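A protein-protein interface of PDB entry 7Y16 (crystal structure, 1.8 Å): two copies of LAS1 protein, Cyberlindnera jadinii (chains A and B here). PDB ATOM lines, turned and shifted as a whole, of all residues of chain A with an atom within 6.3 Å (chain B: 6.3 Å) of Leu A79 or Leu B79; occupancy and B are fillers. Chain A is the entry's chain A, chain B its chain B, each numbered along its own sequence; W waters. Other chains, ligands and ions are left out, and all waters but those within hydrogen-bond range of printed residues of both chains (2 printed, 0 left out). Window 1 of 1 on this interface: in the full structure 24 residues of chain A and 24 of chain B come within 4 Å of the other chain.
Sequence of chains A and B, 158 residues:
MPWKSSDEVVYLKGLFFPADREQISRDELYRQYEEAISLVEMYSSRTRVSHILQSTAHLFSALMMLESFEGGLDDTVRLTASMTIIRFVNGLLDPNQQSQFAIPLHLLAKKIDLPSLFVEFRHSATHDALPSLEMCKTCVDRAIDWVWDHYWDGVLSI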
ATOM      1  N   HIS A  58      -4.955 -27.293  24.602  1.00  0.00           N
ATOM      2  CA  HIS A  58      -4.984 -25.854  24.346  1.00  0.00           C
ATOM      3  C   HIS A  58      -4.788 -25.028  25.626  1.00  0.00           C
ATOM      4  O   HIS A  58      -4.243 -23.922  25.564  1.00  0.00           O
ATOM      5  CB  HIS A  58      -6.283 -25.488  23.645  1.00  0.00           C
ATOM      6  CG  HIS A  58      -6.277 -25.860  22.193  1.00  0.00           C
ATOM      7  ND1 HIS A  58      -7.420 -25.948  21.439  1.00  0.00           N
ATOM      8  CD2 HIS A  58      -5.252 -26.180  21.370  1.00  0.00           C
ATOM      9  CE1 HIS A  58      -7.102 -26.292  20.203  1.00  0.00           C
ATOM     10  NE2 HIS A  58      -5.792 -26.435  20.135  1.00  0.00           N
ATOM     11  N   SER A  61      -1.191 -24.919  25.825  1.00  0.00           N
ATOM     12  CA  SER A  61      -0.747 -23.979  24.794  1.00  0.00           C
ATOM     13  C   SER A  61      -0.852 -22.539  25.297  1.00  0.00           C
ATOM     14  O   SER A  61       0.097 -21.755  25.192  1.00  0.00           O
ATOM     15  CB  SER A  61      -1.562 -24.161  23.505  1.00  0.00           C
ATOM     16  OG  SER A  61      -1.447 -25.500  23.010  1.00  0.00           O
ATOM     17  N   ALA A  62      -1.993 -22.189  25.877  1.00  0.00           N
ATOM     18  CA  ALA A  62      -2.174 -20.836  26.403  1.00  0.00           C
ATOM     19  C   ALA A  62      -1.252 -20.562  27.596  1.00  0.00           C
ATOM     20  O   ALA A  62      -0.735 -19.444  27.738  1.00  0.00           O
ATOM     21  CB  ALA A  62      -3.641 -20.629  26.789  1.00  0.00           C
ATOM     22  N   ASP A  74      -0.345  -7.032  24.670  1.00  0.00           N
ATOM     23  CA  ASP A  74      -0.850  -8.247  25.290  1.00  0.00           C
ATOM     24  C   ASP A  74      -2.043  -8.918  24.588  1.00  0.00           C
ATOM     25  O   ASP A  74      -2.590  -9.878  25.062  1.00  0.00           O
ATOM     26  CB  ASP A  74      -1.135  -8.014  26.781  1.00  0.00           C
ATOM     27  CG  ASP A  74      -2.305  -7.047  27.033  1.00  0.00           C
ATOM     28  OD1 ASP A  74      -2.508  -6.739  28.192  1.00  0.00           O
ATOM     29  OD2 ASP A  74      -2.995  -6.637  26.110  1.00  0.00           O
ATOM     30  N   ASP A  75      -2.451  -8.353  23.470  1.00  0.00           N
ATOM     31  CA  ASP A  75      -3.669  -8.805  22.834  1.00  0.00           C
ATOM     32  C   ASP A  75      -3.644 -10.224  22.333  1.00  0.00           C
ATOM     33  O   ASP A  75      -4.542 -10.951  22.623  1.00  0.00           O
ATOM     34  CB  ASP A  75      -4.138  -7.857  21.730  1.00  0.00           C
ATOM     35  CG  ASP A  75      -3.056  -7.431  20.817  1.00  0.00           C
ATOM     36  OD1 ASP A  75      -3.149  -6.328  20.281  1.00  0.00           O
ATOM     37  OD2 ASP A  75      -2.106  -8.140  20.574  1.00  0.00           O
ATOM     38  N   THR A  76      -2.590 -10.610  21.629  1.00  0.00           N
ATOM     39  CA  THR A  76      -2.587 -11.973  21.094  1.00  0.00           C
ATOM     40  C   THR A  76      -2.603 -13.014  22.212  1.00  0.00           C
ATOM     41  O   THR A  76      -3.266 -14.053  22.077  1.00  0.00           O
ATOM     42  CB  THR A  76      -1.388 -12.191  20.153  1.00  0.00           C
ATOM     43  OG1 THR A  76      -0.158 -12.011  20.866  1.00  0.00           O
ATOM     44  CG2 THR A  76      -1.449 -11.231  18.950  1.00  0.00           C
ATOM     45  N   VAL A  77      -1.939 -12.751  23.343  1.00  0.00           N
ATOM     46  CA  VAL A  77      -1.976 -13.794  24.365  1.00  0.00           C
ATOM     47  C   VAL A  77      -3.343 -13.823  25.028  1.00  0.00           C
ATOM     48  O   VAL A  77      -3.846 -14.895  25.385  1.00  0.00           O
ATOM     49  CB  VAL A  77      -0.835 -13.663  25.391  1.00  0.00           C
ATOM     50  CG1 VAL A  77      -1.026 -12.487  26.316  1.00  0.00           C
ATOM     51  CG2 VAL A  77      -0.725 -14.981  26.189  1.00  0.00           C
ATOM     52  N   ARG A  78      -3.984 -12.661  25.187  1.00  0.00           N
ATOM     53  CA  ARG A  78      -5.333 -12.664  25.737  1.00  0.00           C
ATOM     54  C   ARG A  78      -6.329 -13.261  24.757  1.00  0.00           C
ATOM     55  O   ARG A  78      -7.285 -13.930  25.178  1.00  0.00           O
ATOM     56  CB  ARG A  78      -5.746 -11.243  26.134  1.00  0.00           C
ATOM     57  CG  ARG A  78      -4.951 -10.747  27.354  1.00  0.00           C
ATOM     58  CD  ARG A  78      -5.023  -9.238  27.468  1.00  0.00           C
ATOM     59  NE  ARG A  78      -6.409  -8.779  27.462  1.00  0.00           N
ATOM     60  CZ  ARG A  78      -6.807  -7.587  27.028  1.00  0.00           C
ATOM     61  NH1 ARG A  78      -5.940  -6.734  26.535  1.00  0.00           N
ATOM     62  NH2 ARG A  78      -8.082  -7.241  27.077  1.00  0.00           N
ATOM     63  N   LEU A  79      -6.145 -13.021  23.455  1.00  0.00           N
ATOM     64  CA  LEU A  79      -7.049 -13.640  22.481  1.00  0.00           C
ATOM     65  C   LEU A  79      -6.893 -15.151  22.494  1.00  0.00           C
ATOM     66  O   LEU A  79      -7.885 -15.885  22.484  1.00  0.00           O
ATOM     67  CB  LEU A  79      -6.789 -13.093  21.077  1.00  0.00           C
ATOM     68  CG  LEU A  79      -7.177 -11.622  20.878  1.00  0.00           C
ATOM     69  CD1 LEU A  79      -6.353 -11.081  19.743  1.00  0.00           C
ATOM     70  CD2 LEU A  79      -8.706 -11.482  20.612  1.00  0.00           C
ATOM     71  N   THR A  80      -5.653 -15.633  22.570  1.00  0.00           N
ATOM     72  CA  THR A  80      -5.397 -17.075  22.635  1.00  0.00           C
ATOM     73  C   THR A  80      -6.034 -17.700  23.873  1.00  0.00           C
ATOM     74  O   THR A  80      -6.723 -18.725  23.781  1.00  0.00           O
ATOM     75  CB  THR A  80      -3.887 -17.332  22.637  1.00  0.00           C
ATOM     76  OG1 THR A  80      -3.399 -17.280  21.300  1.00  0.00           O
ATOM     77  CG2 THR A  80      -3.548 -18.710  23.222  1.00  0.00           C
ATOM     78  N   ALA A  81      -5.818 -17.083  25.047  1.00  0.00           N
ATOM     79  CA  ALA A  81      -6.345 -17.647  26.284  1.00  0.00           C
ATOM     80  C   ALA A  81      -7.859 -17.580  26.307  1.00  0.00           C
ATOM     81  O   ALA A  81      -8.517 -18.505  26.806  1.00  0.00           O
ATOM     82  CB  ALA A  81      -5.748 -16.927  27.496  1.00  0.00           C
ATOM     83  N   SER A  82      -8.434 -16.501  25.769  1.00  0.00           N
ATOM     84  CA  SER A  82      -9.885 -16.371  25.781  1.00  0.00           C
ATOM     85  C   SER A  82     -10.538 -17.412  24.883  1.00  0.00           C
ATOM     86  O   SER A  82     -11.594 -17.954  25.232  1.00  0.00           O
ATOM     87  CB  SER A  82     -10.290 -14.967  25.353  1.00  0.00           C
ATOM     88  OG  SER A  82      -9.923 -14.032  26.375  1.00  0.00           O
ATOM     89  N   MET A  83      -9.953 -17.677  23.712  1.00  0.00           N
ATOM     90  CA  MET A  83     -10.523 -18.697  22.826  1.00  0.00           C
ATOM     91  C   MET A  83     -10.493 -20.065  23.492  1.00  0.00           C
ATOM     92  O   MET A  83     -11.444 -20.857  23.377  1.00  0.00           O
ATOM     93  CB  MET A  83      -9.755 -18.755  21.508  1.00  0.00           C
ATOM     94  CG  MET A  83     -10.408 -19.648  20.458  1.00  0.00           C
ATOM     95  SD  MET A  83     -11.906 -18.925  19.742  1.00  0.00           S
ATOM     96  CE  MET A  83     -13.228 -19.652  20.740  1.00  0.00           C
ATOM     97  N   THR A  84      -9.389 -20.362  24.172  1.00  0.00           N
ATOM     98  CA  THR A  84      -9.231 -21.626  24.880  1.00  0.00           C
ATOM     99  C   THR A  84     -10.317 -21.818  25.933  1.00  0.00           C
ATOM    100  O   THR A  84     -10.937 -22.891  26.011  1.00  0.00           O
ATOM    101  CB  THR A  84      -7.840 -21.669  25.512  1.00  0.00           C
ATOM    102  OG1 THR A  84      -6.865 -21.615  24.462  1.00  0.00           O
ATOM    103  CG2 THR A  84      -7.653 -22.952  26.286  1.00  0.00           C
ATOM    104  N   ARG A  87     -13.852 -22.433  24.358  1.00  0.00           N
ATOM    105  CA  ARG A  87     -14.038 -23.762  23.789  1.00  0.00           C
ATOM    106  C   ARG A  87     -14.095 -24.813  24.896  1.00  0.00           C
ATOM    107  O   ARG A  87     -14.847 -25.789  24.796  1.00  0.00           O
ATOM    108  CB  ARG A  87     -12.913 -24.054  22.775  1.00  0.00           C
ATOM    109  CG  ARG A  87     -13.004 -23.194  21.482  1.00  0.00           C
ATOM    110  CD  ARG A  87     -11.821 -23.425  20.528  1.00  0.00           C
ATOM    111  NE  ARG A  87     -11.698 -24.848  20.213  1.00  0.00           N
ATOM    112  CZ  ARG A  87     -12.375 -25.488  19.257  1.00  0.00           C
ATOM    113  NH1 ARG A  87     -13.222 -24.839  18.455  1.00  0.00           N
ATOM    114  NH2 ARG A  87     -12.198 -26.798  19.107  1.00  0.00           N
ATOM    115  N   LEU A 130     -12.554  -7.791  26.056  1.00  0.00           N
ATOM    116  CA  LEU A 130     -11.713  -8.956  26.119  1.00  0.00           C
ATOM    117  C   LEU A 130     -11.112  -9.011  27.527  1.00  0.00           C
ATOM    118  O   LEU A 130     -10.580  -8.044  27.990  1.00  0.00           O
ATOM    119  CB  LEU A 130     -10.625  -8.847  25.065  1.00  0.00           C
ATOM    120  CG  LEU A 130      -9.714 -10.047  24.859  1.00  0.00           C
ATOM    121  CD1 LEU A 130     -10.433 -11.240  24.278  1.00  0.00           C
ATOM    122  CD2 LEU A 130      -8.454  -9.715  24.105  1.00  0.00           C
ATOM    123  N   CYS A 136      -7.077 -13.702  32.323  1.00  0.00           N
ATOM    124  CA  CYS A 136      -6.749 -14.855  31.483  1.00  0.00           C
ATOM    125  C   CYS A 136      -5.821 -15.821  32.204  1.00  0.00           C
ATOM    126  O   CYS A 136      -5.999 -17.048  32.138  1.00  0.00           O
ATOM    127  CB  CYS A 136      -6.094 -14.370  30.186  1.00  0.00           C
ATOM    128  SG  CYS A 136      -7.287 -13.573  29.012  1.00  0.00           S
ATOM    129  N   HIS B  58      -7.458  -5.703  16.630  1.00  0.00           N
ATOM    130  CA  HIS B  58      -7.187  -7.122  16.867  1.00  0.00           C
ATOM    131  C   HIS B  58      -6.971  -7.892  15.565  1.00  0.00           C
ATOM    132  O   HIS B  58      -6.172  -8.847  15.533  1.00  0.00           O
ATOM    133  CB  HIS B  58      -8.336  -7.745  17.676  1.00  0.00           C
ATOM    134  CG  HIS B  58      -8.312  -7.373  19.129  1.00  0.00           C
ATOM    135  ND1 HIS B  58      -9.417  -7.475  19.944  1.00  0.00           N
ATOM    136  CD2 HIS B  58      -7.311  -6.892  19.906  1.00  0.00           C
ATOM    137  CE1 HIS B  58      -9.100  -7.076  21.162  1.00  0.00           C
ATOM    138  NE2 HIS B  58      -7.830  -6.713  21.163  1.00  0.00           N
ATOM    139  N   SER B  61      -3.416  -7.376  14.705  1.00  0.00           N
ATOM    140  CA  SER B  61      -2.656  -8.207  15.641  1.00  0.00           C
ATOM    141  C   SER B  61      -2.646  -9.668  15.204  1.00  0.00           C
ATOM    142  O   SER B  61      -1.611 -10.344  15.276  1.00  0.00           O
ATOM    143  CB  SER B  61      -3.242  -8.101  17.053  1.00  0.00           C
ATOM    144  OG  SER B  61      -2.899  -6.891  17.682  1.00  0.00           O
ATOM    145  N   ALA B  62      -3.808 -10.189  14.788  1.00  0.00           N
ATOM    146  CA  ALA B  62      -3.873 -11.572  14.324  1.00  0.00           C
ATOM    147  C   ALA B  62      -3.123 -11.745  13.011  1.00  0.00           C
ATOM    148  O   ALA B  62      -2.454 -12.761  12.797  1.00  0.00           O
ATOM    149  CB  ALA B  62      -5.326 -12.011  14.146  1.00  0.00           C
ATOM    150  N   ASP B  74       0.838 -24.915  15.613  1.00  0.00           N
ATOM    151  CA  ASP B  74       0.102 -23.759  15.113  1.00  0.00           C
ATOM    152  C   ASP B  74      -1.088 -23.385  15.989  1.00  0.00           C
ATOM    153  O   ASP B  74      -1.844 -22.470  15.637  1.00  0.00           O
ATOM    154  CB  ASP B  74      -0.346 -24.011  13.668  1.00  0.00           C
ATOM    155  CG  ASP B  74      -1.339 -25.176  13.527  1.00  0.00           C
ATOM    156  OD1 ASP B  74      -1.787 -25.750  14.535  1.00  0.00           O
ATOM    157  OD2 ASP B  74      -1.680 -25.507  12.368  1.00  0.00           O
ATOM    158  N   ASP B  75      -1.247 -24.030  17.147  1.00  0.00           N
ATOM    159  CA  ASP B  75      -2.484 -23.840  17.901  1.00  0.00           C
ATOM    160  C   ASP B  75      -2.670 -22.393  18.353  1.00  0.00           C
ATOM    161  O   ASP B  75      -3.769 -21.854  18.226  1.00  0.00           O
ATOM    162  CB  ASP B  75      -2.542 -24.796  19.086  1.00  0.00           C
ATOM    163  CG  ASP B  75      -2.383 -26.229  18.650  1.00  0.00           C
ATOM    164  OD1 ASP B  75      -3.393 -26.938  18.497  1.00  0.00           O
ATOM    165  OD2 ASP B  75      -1.236 -26.615  18.395  1.00  0.00           O
ATOM    166  N   THR B  76      -1.619 -21.741  18.863  1.00  0.00           N
ATOM    167  CA  THR B  76      -1.830 -20.413  19.448  1.00  0.00           C
ATOM    168  C   THR B  76      -2.183 -19.376  18.390  1.00  0.00           C
ATOM    169  O   THR B  76      -3.029 -18.505  18.632  1.00  0.00           O
ATOM    170  CB  THR B  76      -0.616 -19.965  20.261  1.00  0.00           C
ATOM    171  OG1 THR B  76       0.550 -19.870  19.440  1.00  0.00           O
ATOM    172  CG2 THR B  76      -0.370 -20.917  21.469  1.00  0.00           C
ATOM    173  N   VAL B  77      -1.595 -19.463  17.193  1.00  0.00           N
ATOM    174  CA  VAL B  77      -1.964 -18.476  16.175  1.00  0.00           C
ATOM    175  C   VAL B  77      -3.400 -18.696  15.722  1.00  0.00           C
ATOM    176  O   VAL B  77      -4.120 -17.733  15.420  1.00  0.00           O
ATOM    177  CB  VAL B  77      -0.971 -18.485  14.989  1.00  0.00           C
ATOM    178  CG1 VAL B  77      -0.958 -19.807  14.272  1.00  0.00           C
ATOM    179  CG2 VAL B  77      -1.310 -17.373  13.993  1.00  0.00           C
ATOM    180  N   ARG B  78      -3.835 -19.969  15.654  1.00  0.00           N
ATOM    181  CA  ARG B  78      -5.214 -20.277  15.288  1.00  0.00           C
ATOM    182  C   ARG B  78      -6.184 -19.838  16.377  1.00  0.00           C
ATOM    183  O   ARG B  78      -7.263 -19.318  16.073  1.00  0.00           O
ATOM    184  CB  ARG B  78      -5.368 -21.783  15.012  1.00  0.00           C
ATOM    185  CG  ARG B  78      -4.750 -22.187  13.668  1.00  0.00           C
ATOM    186  CD  ARG B  78      -4.442 -23.658  13.620  1.00  0.00           C
ATOM    187  NE  ARG B  78      -5.670 -24.433  13.682  1.00  0.00           N
ATOM    188  CZ  ARG B  78      -5.757 -25.634  14.229  1.00  0.00           C
ATOM    189  NH1 ARG B  78      -4.673 -26.187  14.764  1.00  0.00           N
ATOM    190  NH2 ARG B  78      -6.928 -26.260  14.245  1.00  0.00           N
ATOM    191  N   LEU B  79      -5.827 -20.059  17.644  1.00  0.00           N
ATOM    192  CA  LEU B  79      -6.690 -19.613  18.737  1.00  0.00           C
ATOM    193  C   LEU B  79      -6.812 -18.092  18.738  1.00  0.00           C
ATOM    194  O   LEU B  79      -7.918 -17.548  18.872  1.00  0.00           O
ATOM    195  CB  LEU B  79      -6.135 -20.120  20.073  1.00  0.00           C
ATOM    196  CG  LEU B  79      -6.155 -21.638  20.292  1.00  0.00           C
ATOM    197  CD1 LEU B  79      -5.113 -22.069  21.359  1.00  0.00           C
ATOM    198  CD2 LEU B  79      -7.580 -22.072  20.670  1.00  0.00           C
ATOM    199  N   THR B  80      -5.686 -17.394  18.554  1.00  0.00           N
ATOM    200  CA  THR B  80      -5.694 -15.932  18.436  1.00  0.00           C
ATOM    201  C   THR B  80      -6.610 -15.463  17.308  1.00  0.00           C
ATOM    202  O   THR B  80      -7.488 -14.615  17.510  1.00  0.00           O
ATOM    203  CB  THR B  80      -4.268 -15.433  18.200  1.00  0.00           C
ATOM    204  OG1 THR B  80      -3.507 -15.570  19.398  1.00  0.00           O
ATOM    205  CG2 THR B  80      -4.262 -13.966  17.761  1.00  0.00           C
ATOM    206  N   ALA B  81      -6.405 -15.995  16.101  1.00  0.00           N
ATOM    207  CA  ALA B  81      -7.189 -15.564  14.953  1.00  0.00           C
ATOM    208  C   ALA B  81      -8.663 -15.889  15.133  1.00  0.00           C
ATOM    209  O   ALA B  81      -9.531 -15.081  14.781  1.00  0.00           O
ATOM    210  CB  ALA B  81      -6.643 -16.214  13.676  1.00  0.00           C
ATOM    211  N   SER B  82      -8.967 -17.074  15.672  1.00  0.00           N
ATOM    212  CA  SER B  82     -10.356 -17.487  15.827  1.00  0.00           C
ATOM    213  C   SER B  82     -11.087 -16.572  16.791  1.00  0.00           C
ATOM    214  O   SER B  82     -12.258 -16.242  16.577  1.00  0.00           O
ATOM    215  CB  SER B  82     -10.420 -18.945  16.309  1.00  0.00           C
ATOM    216  OG  SER B  82     -10.065 -19.832  15.258  1.00  0.00           O
ATOM    217  N   MET B  83     -10.440 -16.197  17.896  1.00  0.00           N
ATOM    218  CA  MET B  83     -11.099 -15.316  18.856  1.00  0.00           C
ATOM    219  C   MET B  83     -11.373 -13.953  18.232  1.00  0.00           C
ATOM    220  O   MET B  83     -12.420 -13.339  18.476  1.00  0.00           O
ATOM    221  CB  MET B  83     -10.235 -15.143  20.110  1.00  0.00           C
ATOM    222  CG  MET B  83     -10.911 -14.349  21.241  1.00  0.00           C
ATOM    223  SD  MET B  83     -12.150 -15.267  22.175  1.00  0.00           S
ATOM    224  CE  MET B  83     -13.704 -14.986  21.308  1.00  0.00           C
ATOM    225  N   THR B  84     -10.436 -13.474  17.418  1.00  0.00           N
ATOM    226  CA  THR B  84     -10.607 -12.190  16.749  1.00  0.00           C
ATOM    227  C   THR B  84     -11.819 -12.217  15.824  1.00  0.00           C
ATOM    228  O   THR B  84     -12.652 -11.301  15.836  1.00  0.00           O
ATOM    229  CB  THR B  84      -9.341 -11.850  15.970  1.00  0.00           C
ATOM    230  OG1 THR B  84      -8.210 -11.807  16.862  1.00  0.00           O
ATOM    231  CG2 THR B  84      -9.480 -10.484  15.264  1.00  0.00           C
ATOM    232  N   ARG B  87     -15.232 -12.273  17.730  1.00  0.00           N
ATOM    233  CA  ARG B  87     -15.638 -10.995  18.308  1.00  0.00           C
ATOM    234  C   ARG B  87     -16.005  -9.990  17.224  1.00  0.00           C
ATOM    235  O   ARG B  87     -16.940  -9.192  17.393  1.00  0.00           O
ATOM    236  CB  ARG B  87     -14.518 -10.460  19.189  1.00  0.00           C
ATOM    237  CG  ARG B  87     -14.401 -11.222  20.520  1.00  0.00           C
ATOM    238  CD  ARG B  87     -13.138 -10.816  21.243  1.00  0.00           C
ATOM    239  NE  ARG B  87     -13.190  -9.397  21.590  1.00  0.00           N
ATOM    240  CZ  ARG B  87     -13.782  -8.926  22.682  1.00  0.00           C
ATOM    241  NH1 ARG B  87     -14.366  -9.752  23.536  1.00  0.00           N
ATOM    242  NH2 ARG B  87     -13.803  -7.623  22.903  1.00  0.00           N
ATOM    243  N   LEU B 130     -11.442 -26.405  15.729  1.00  0.00           N
ATOM    244  CA  LEU B 130     -10.815 -25.117  15.563  1.00  0.00           C
ATOM    245  C   LEU B 130     -10.369 -24.986  14.106  1.00  0.00           C
ATOM    246  O   LEU B 130      -9.712 -25.815  13.593  1.00  0.00           O
ATOM    247  CB  LEU B 130      -9.605 -25.010  16.452  1.00  0.00           C
ATOM    248  CG  LEU B 130      -8.850 -23.703  16.549  1.00  0.00           C
ATOM    249  CD1 LEU B 130      -9.676 -22.566  17.117  1.00  0.00           C
ATOM    250  CD2 LEU B 130      -7.518 -23.898  17.246  1.00  0.00           C
ATOM    251  N   CYS B 136      -7.945 -19.590   9.019  1.00  0.00           N
ATOM    252  CA  CYS B 136      -7.723 -18.391   9.820  1.00  0.00           C
ATOM    253  C   CYS B 136      -7.151 -17.254   8.978  1.00  0.00           C
ATOM    254  O   CYS B 136      -7.605 -16.109   9.077  1.00  0.00           O
ATOM    255  CB  CYS B 136      -6.791 -18.719  10.985  1.00  0.00           C
ATOM    256  SG  CYS B 136      -7.611 -19.652  12.294  1.00  0.00           S
HETATM  257  O   HOH W   1       0.046  -7.698  18.695  1.00  0.00           O
HETATM  258  O   HOH W   2       0.273 -25.521  20.849  1.00  0.00           O
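Leu B79 touches its own counterpart, Leu A79.
Leu A79 touches Thr B84, and with the chains exchanged Thr A84 touches Leu B79.
Ser A82 touches Met B83, and with the chains exchanged Met A83 touches Ser B82.
Met B83 touches its own counterpart, Met A83.
Positions printed for both chains: 58, 61, 62, 74, 75, 76, 77, 78, 79, 80, 81, 82, 83, 84, 87, 130 and 136.
Water W2 lies within hydrogen-bond range of OG of Ser A61 (2.8 Å) and OD2 of Asp B75 (3.1 Å).
Water W1 bridges the side-chain carboxylate (OD2) of Asp A75 (2.9 Å) and the side-chain hydroxyl (OG) of Ser B61 (3.2 Å).
Of the printed residues of chain A, Leu B79 touches His A58 (3.95 Å), Leu A79 (3.98 Å), Met A83 (3.4 Å) and Thr A84 (3.6 Å).
Printed residues of chain B within 4 Å of Leu A130: Arg B87.
Printed residues of chain B within 4 Å of Asp A75: His B58 and Ser B61.
Of the printed residues of chain A, Met B83 touches Leu A79 (3.4 Å), Ser A82 (3.7 Å) and Met A83 (3.6 Å).
Of the printed residues of chain B, His A58 touches Asp B75, Leu B79 and Leu B130.
Asp B74 touches none of the printed residues of chain A.
Cys B136 touches none of the printed residues of chain A.
The nearest residue of chain B that does not touch Leu A79 is His B58 (4.1 Å).
The nearest printed residue of chain A that does not touch Leu B130 is Met A83 (4.5 Å).
Among the printed residues, merely in contact across the chains: Leu A79 with Met B83, Met A83 with Leu B79, Leu A79 with Thr B84, Thr A84 with Leu B79, Ser A82 with Met B83, Met A83 with Ser B82, Thr A76 with Ser B61, Asp A75 with His B58, His A58 with Leu B130, Ser A61 with Thr B76, Leu A79 with Thr B80, His A58 with Leu B79 and Leu A79 with Leu B79.
OG of Ser B82 lies within hydrogen-bond range of O of Arg B78, 3.0 Å away.
O of Thr B76 is in hydrogen-bond range of OG1 of Thr B80, 3.1 Å away.
The backbone carbonyl oxygen (O) of Thr A76 lies within hydrogen-bond range of the side-chain hydroxyl (OG1) of Thr A80 (3.3 Å).
NH2 of Arg A78 lies within hydrogen-bond range of O of Leu A130 (2.8 Å).
OG of Ser A82 lies within hydrogen-bond range of SG of Cys A136 (3.8 Å).
The backbone carbonyl oxygen of Thr A80 lies within hydrogen-bond range of the side-chain hydroxyl of Thr A84, 3.0 Å away.
The backbone carbonyl oxygen (O) of Thr A76 sits at hydrogen-bond distance from the side-chain hydroxyl (OG1) of Thr B80, 3.1 Å away.
The backbone carbonyl oxygen (O) of Thr B76 lies within hydrogen-bond range of the side-chain hydroxyl (OG1) of Thr A80, 3.0 Å away.
A ring nitrogen (NE2) of His A58 lies within hydrogen-bond range of the side-chain carboxylate (OD1) of Asp B75, at 2.9 Å.
The side-chain hydroxyl of Thr B80 lies within hydrogen-bond range of the side-chain hydroxyl of Thr A80.
The guanidinium group of Arg A87 sits close to the backbone NH of Leu B130, 3.5 Å away.
The side-chain carboxylate of Asp A75 lies within hydrogen-bond range of the side-chain hydroxyl of Ser B61, at 2.7 Å.
N of Leu A130 lies close to NH2 of Arg B87, at 3.4 Å.
The backbone NH (N) of Met A83 sits at hydrogen-bond distance from the side-chain sulfur (SD) of Met B83 (3.6 Å).
Along chain B the printed residues that touch a printed residue of chain A span positions 58 to 130.
Of the 17 printed residues of chain A, 11 touch a printed residue of chain B.
Hydrophobic or aromatic side chains of chain A that line the printed part of chain B: His A58, Leu A79, Met A83 and Leu A130.
Among the printed residues, 21 pairs touch across the chains.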
